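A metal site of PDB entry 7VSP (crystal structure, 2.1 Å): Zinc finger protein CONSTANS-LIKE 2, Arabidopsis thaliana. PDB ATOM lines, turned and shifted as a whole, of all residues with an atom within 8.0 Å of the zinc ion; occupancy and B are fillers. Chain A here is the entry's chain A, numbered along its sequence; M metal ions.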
ATOM      1  N   LEU A  71     -13.637 -10.679   0.278  1.00  0.00           N
ATOM      2  CA  LEU A  71     -13.989 -11.633  -0.761  1.00  0.00           C
ATOM      3  C   LEU A  71     -15.446 -11.403  -1.149  1.00  0.00           C
ATOM      4  O   LEU A  71     -16.326 -11.405  -0.280  1.00  0.00           O
ATOM      5  CB  LEU A  71     -13.764 -13.067  -0.255  1.00  0.00           C
ATOM      6  CG  LEU A  71     -13.923 -14.271  -1.202  1.00  0.00           C
ATOM      7  CD1 LEU A  71     -15.330 -14.771  -1.135  1.00  0.00           C
ATOM      8  CD2 LEU A  71     -13.567 -13.969  -2.630  1.00  0.00           C
ATOM      9  N   CYS A  72     -15.690 -11.201  -2.434  1.00  0.00           N
ATOM     10  CA  CYS A  72     -17.086 -11.095  -2.894  1.00  0.00           C
ATOM     11  C   CYS A  72     -17.385 -12.326  -3.755  1.00  0.00           C
ATOM     12  O   CYS A  72     -16.880 -12.417  -4.848  1.00  0.00           O
ATOM     13  CB  CYS A  72     -17.343  -9.816  -3.688  1.00  0.00           C
ATOM     14  SG  CYS A  72     -19.034  -9.731  -4.290  1.00  0.00           S
ATOM     15  N   LYS A  73     -18.261 -13.185  -3.274  1.00  0.00           N
ATOM     16  CA  LYS A  73     -18.562 -14.402  -4.023  1.00  0.00           C
ATOM     17  C   LYS A  73     -19.398 -14.094  -5.242  1.00  0.00           C
ATOM     18  O   LYS A  73     -19.221 -14.721  -6.295  1.00  0.00           O
ATOM     19  CB  LYS A  73     -19.264 -15.414  -3.134  1.00  0.00           C
ATOM     20  CG  LYS A  73     -18.281 -16.289  -2.307  1.00  0.00           C
ATOM     21  CD  LYS A  73     -18.696 -16.397  -0.823  1.00  0.00           C
ATOM     22  CE  LYS A  73     -19.179 -17.803  -0.481  1.00  0.00           C
ATOM     23  NZ  LYS A  73     -18.726 -18.267   0.877  1.00  0.00           N
ATOM     24  N   ALA A  74     -20.301 -13.115  -5.134  1.00  0.00           N
ATOM     25  CA  ALA A  74     -21.077 -12.690  -6.305  1.00  0.00           C
ATOM     26  C   ALA A  74     -20.159 -12.276  -7.458  1.00  0.00           C
ATOM     27  O   ALA A  74     -20.360 -12.705  -8.604  1.00  0.00           O
ATOM     28  CB  ALA A  74     -22.023 -11.538  -5.914  1.00  0.00           C
ATOM     29  N   ASP A  75     -19.150 -11.446  -7.179  1.00  0.00           N
ATOM     30  CA  ASP A  75     -18.188 -11.057  -8.221  1.00  0.00           C
ATOM     31  C   ASP A  75     -17.082 -12.081  -8.431  1.00  0.00           C
ATOM     32  O   ASP A  75     -16.269 -11.887  -9.332  1.00  0.00           O
ATOM     33  CB  ASP A  75     -17.549  -9.703  -7.891  1.00  0.00           C
ATOM     34  CG  ASP A  75     -18.498  -8.530  -8.052  1.00  0.00           C
ATOM     35  OD1 ASP A  75     -19.211  -8.475  -9.057  1.00  0.00           O
ATOM     36  OD2 ASP A  75     -18.550  -7.669  -7.150  1.00  0.00           O
ATOM     37  N   ALA A  76     -17.016 -13.145  -7.628  1.00  0.00           N
ATOM     38  CA  ALA A  76     -15.922 -14.130  -7.668  1.00  0.00           C
ATOM     39  C   ALA A  76     -14.551 -13.442  -7.626  1.00  0.00           C
ATOM     40  O   ALA A  76     -13.661 -13.721  -8.443  1.00  0.00           O
ATOM     41  CB  ALA A  76     -16.037 -15.055  -8.882  1.00  0.00           C
ATOM     42  N   ALA A  77     -14.382 -12.545  -6.654  1.00  0.00           N
ATOM     43  CA  ALA A  77     -13.223 -11.655  -6.623  1.00  0.00           C
ATOM     44  C   ALA A  77     -12.806 -11.344  -5.195  1.00  0.00           C
ATOM     45  O   ALA A  77     -13.641 -11.022  -4.343  1.00  0.00           O
ATOM     46  CB  ALA A  77     -13.529 -10.360  -7.376  1.00  0.00           C
ATOM     47  N   LEU A  79     -10.840  -8.523  -3.252  1.00  0.00           N
ATOM     48  CA  LEU A  79     -10.601  -7.112  -3.514  1.00  0.00           C
ATOM     49  C   LEU A  79      -9.907  -6.412  -2.343  1.00  0.00           C
ATOM     50  O   LEU A  79     -10.242  -6.640  -1.181  1.00  0.00           O
ATOM     51  CB  LEU A  79     -11.916  -6.400  -3.811  1.00  0.00           C
ATOM     52  CG  LEU A  79     -12.825  -7.056  -4.848  1.00  0.00           C
ATOM     53  CD1 LEU A  79     -14.263  -6.450  -4.807  1.00  0.00           C
ATOM     54  CD2 LEU A  79     -12.154  -6.890  -6.212  1.00  0.00           C
ATOM     55  N   ASP A  84     -12.695  -2.624  -3.205  1.00  0.00           N
ATOM     56  CA  ASP A  84     -13.969  -3.061  -2.652  1.00  0.00           C
ATOM     57  C   ASP A  84     -14.953  -1.904  -2.539  1.00  0.00           C
ATOM     58  O   ASP A  84     -16.145  -2.065  -2.787  1.00  0.00           O
ATOM     59  CB  ASP A  84     -13.792  -3.713  -1.268  1.00  0.00           C
ATOM     60  CG  ASP A  84     -15.116  -4.146  -0.669  1.00  0.00           C
ATOM     61  OD1 ASP A  84     -15.743  -5.096  -1.199  1.00  0.00           O
ATOM     62  OD2 ASP A  84     -15.547  -3.540   0.336  1.00  0.00           O
ATOM     63  N   ILE A  87     -15.887  -0.645  -6.333  1.00  0.00           N
ATOM     64  CA  ILE A  87     -16.751  -1.553  -7.091  1.00  0.00           C
ATOM     65  C   ILE A  87     -18.163  -1.586  -6.515  1.00  0.00           C
ATOM     66  O   ILE A  87     -19.148  -1.568  -7.268  1.00  0.00           O
ATOM     67  CB  ILE A  87     -16.098  -2.946  -7.149  1.00  0.00           C
ATOM     68  CG1 ILE A  87     -14.981  -2.922  -8.209  1.00  0.00           C
ATOM     69  CG2 ILE A  87     -17.140  -4.062  -7.369  1.00  0.00           C
ATOM     70  CD1 ILE A  87     -14.101  -4.128  -8.182  1.00  0.00           C
ATOM     71  N   HIS A  88     -18.290  -1.618  -5.198  1.00  0.00           N
ATOM     72  CA  HIS A  88     -19.611  -1.797  -4.615  1.00  0.00           C
ATOM     73  C   HIS A  88     -20.377  -0.514  -4.362  1.00  0.00           C
ATOM     74  O   HIS A  88     -21.520  -0.575  -3.912  1.00  0.00           O
ATOM     75  CB  HIS A  88     -19.500  -2.628  -3.343  1.00  0.00           C
ATOM     76  CG  HIS A  88     -18.933  -3.978  -3.641  1.00  0.00           C
ATOM     77  ND1 HIS A  88     -17.669  -4.367  -3.272  1.00  0.00           N
ATOM     78  CD2 HIS A  88     -19.456  -4.997  -4.356  1.00  0.00           C
ATOM     79  CE1 HIS A  88     -17.449  -5.595  -3.704  1.00  0.00           C
ATOM     80  NE2 HIS A  88     -18.523  -6.005  -4.351  1.00  0.00           N
ATOM     81  N   MET A  93     -27.239  -2.478  -7.630  1.00  0.00           N
ATOM     82  CA  MET A  93     -27.009  -3.922  -7.632  1.00  0.00           C
ATOM     83  C   MET A  93     -25.691  -4.271  -6.965  1.00  0.00           C
ATOM     84  O   MET A  93     -25.612  -5.242  -6.211  1.00  0.00           O
ATOM     85  CB  MET A  93     -27.027  -4.490  -9.048  1.00  0.00           C
ATOM     86  CG  MET A  93     -28.312  -4.134  -9.741  1.00  0.00           C
ATOM     87  SD  MET A  93     -29.788  -5.183  -8.937  1.00  0.00           S
ATOM     88  CE  MET A  93     -30.588  -3.695  -7.833  1.00  0.00           C
ATOM     89  N   ALA A  94     -24.638  -3.528  -7.310  1.00  0.00           N
ATOM     90  CA  ALA A  94     -23.346  -3.757  -6.681  1.00  0.00           C
ATOM     91  C   ALA A  94     -23.414  -3.467  -5.186  1.00  0.00           C
ATOM     92  O   ALA A  94     -22.767  -4.162  -4.405  1.00  0.00           O
ATOM     93  CB  ALA A  94     -22.275  -2.882  -7.346  1.00  0.00           C
ATOM     94  N   ARG A  95     -24.193  -2.461  -4.802  1.00  0.00           N
ATOM     95  CA  ARG A  95     -24.309  -2.003  -3.391  1.00  0.00           C
ATOM     96  C   ARG A  95     -24.821  -3.137  -2.493  1.00  0.00           C
ATOM     97  O   ARG A  95     -24.428  -3.172  -1.362  1.00  0.00           O
ATOM     98  CB  ARG A  95     -25.122  -0.713  -3.274  1.00  0.00           C
ATOM     99  CG  ARG A  95     -24.360   0.582  -3.446  1.00  0.00           C
ATOM    100  CD  ARG A  95     -25.208   1.832  -3.601  1.00  0.00           C
ATOM    101  NE  ARG A  95     -24.639   2.892  -4.428  1.00  0.00           N
ATOM    102  CZ  ARG A  95     -25.242   3.481  -5.458  1.00  0.00           C
ATOM    103  NH1 ARG A  95     -26.464   3.149  -5.800  1.00  0.00           N
ATOM    104  NH2 ARG A  95     -24.632   4.430  -6.139  1.00  0.00           N
ATOM    105  N   ARG A  96     -25.652  -4.042  -3.001  1.00  0.00           N
ATOM    106  CA  ARG A  96     -26.187  -5.116  -2.117  1.00  0.00           C
ATOM    107  C   ARG A  96     -25.255  -6.311  -1.980  1.00  0.00           C
ATOM    108  O   ARG A  96     -25.624  -7.228  -1.269  1.00  0.00           O
ATOM    109  CB  ARG A  96     -27.592  -5.584  -2.512  1.00  0.00           C
ATOM    110  CG  ARG A  96     -27.764  -6.137  -3.899  1.00  0.00           C
ATOM    111  CD  ARG A  96     -29.163  -6.662  -4.145  1.00  0.00           C
ATOM    112  NE  ARG A  96     -29.277  -7.232  -5.472  1.00  0.00           N
ATOM    113  CZ  ARG A  96     -30.380  -7.714  -6.003  1.00  0.00           C
ATOM    114  NH1 ARG A  96     -31.502  -7.728  -5.328  1.00  0.00           N
ATOM    115  NH2 ARG A  96     -30.349  -8.196  -7.222  1.00  0.00           N
ATOM    116  N   HIS A  97     -24.100  -6.321  -2.644  1.00  0.00           N
ATOM    117  CA  HIS A  97     -23.241  -7.490  -2.533  1.00  0.00           C
ATOM    118  C   HIS A  97     -22.750  -7.645  -1.099  1.00  0.00           C
ATOM    119  O   HIS A  97     -22.265  -6.677  -0.489  1.00  0.00           O
ATOM    120  CB  HIS A  97     -22.031  -7.392  -3.463  1.00  0.00           C
ATOM    121  CG  HIS A  97     -22.373  -7.521  -4.905  1.00  0.00           C
ATOM    122  ND1 HIS A  97     -21.424  -7.553  -5.888  1.00  0.00           N
ATOM    123  CD2 HIS A  97     -23.566  -7.605  -5.540  1.00  0.00           C
ATOM    124  CE1 HIS A  97     -21.997  -7.664  -7.075  1.00  0.00           C
ATOM    125  NE2 HIS A  97     -23.307  -7.693  -6.889  1.00  0.00           N
ATOM    126  N   GLN A  98     -22.861  -8.867  -0.595  1.00  0.00           N
ATOM    127  CA  GLN A  98     -22.342  -9.253   0.715  1.00  0.00           C
ATOM    128  C   GLN A  98     -20.915  -9.741   0.539  1.00  0.00           C
ATOM    129  O   GLN A  98     -20.657 -10.581  -0.336  1.00  0.00           O
ATOM    130  CB  GLN A  98     -23.233 -10.344   1.322  1.00  0.00           C
ATOM    131  CG  GLN A  98     -24.702  -9.941   1.518  1.00  0.00           C
ATOM    132  CD  GLN A  98     -24.888  -8.995   2.672  1.00  0.00           C
ATOM    133  OE1 GLN A  98     -24.022  -8.933   3.593  1.00  0.00           O
ATOM    134  NE2 GLN A  98     -25.978  -8.243   2.651  1.00  0.00           N
ATOM    135  N   ARG A  99     -20.035  -9.166   1.303  1.00  0.00           N
ATOM    136  CA  ARG A  99     -18.637  -9.570   1.228  1.00  0.00           C
ATOM    137  C   ARG A  99     -18.133 -10.117   2.554  1.00  0.00           C
ATOM    138  O   ARG A  99     -18.637  -9.775   3.601  1.00  0.00           O
ATOM    139  CB  ARG A  99     -17.727  -8.460   0.658  1.00  0.00           C
ATOM    140  CG  ARG A  99     -18.008  -8.029  -0.765  1.00  0.00           C
ATOM    141  CD  ARG A  99     -19.024  -6.914  -0.830  1.00  0.00           C
ATOM    142  NE  ARG A  99     -18.484  -5.664  -0.358  1.00  0.00           N
ATOM    143  CZ  ARG A  99     -19.189  -4.563  -0.165  1.00  0.00           C
ATOM    144  NH1 ARG A  99     -20.488  -4.556  -0.405  1.00  0.00           N
ATOM    145  NH2 ARG A  99     -18.607  -3.474   0.269  1.00  0.00           N
HETATM  146 ZN    ZN M   1     -19.335  -7.680  -5.312  1.00  0.00          ZN
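Four residues have an atom within 4 Å of the zinc ion: Cys 72, Asp 75, His 88 and His 97.
Along chain A the residues within 4 Å of the zinc ion span positions 72 to 97.
OD2 of Asp 75 binds the zinc ion (2.0 Å).
The zinc ion is bound by NE2 of His 88 (2.1 Å).
ND1 of His 97 is bound to the zinc ion, at 2.2 Å.
The side-chain sulfur (SG) of Cys 72 is bound to the zinc ion, 2.3 Å away.
The zinc ion has four donor atoms within binding distance.
O of His 88 lies close to N of Arg 95, at 3.4 Å.
A ring nitrogen (ND1) of His 88 is in hydrogen-bond range of the guanidinium group (NE) of Arg 99, at 3.3 Å.
The backbone NH (N) of Ala 74 sits close to the side-chain sulfur (SG) of Cys 72.
ND1 of His 88 lies within hydrogen-bond range of O of Asp 84.
A ring nitrogen (NE2) of His 97 lies close to the backbone carbonyl oxygen (O) of Met 93, at 3.4 Å.
The backbone NH (N) of Cys 72 is in hydrogen-bond range of the backbone carbonyl oxygen (O) of Ala 77.
O of His 97 is in hydrogen-bond range of NH1 of Arg 99, 2.8 Å away.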
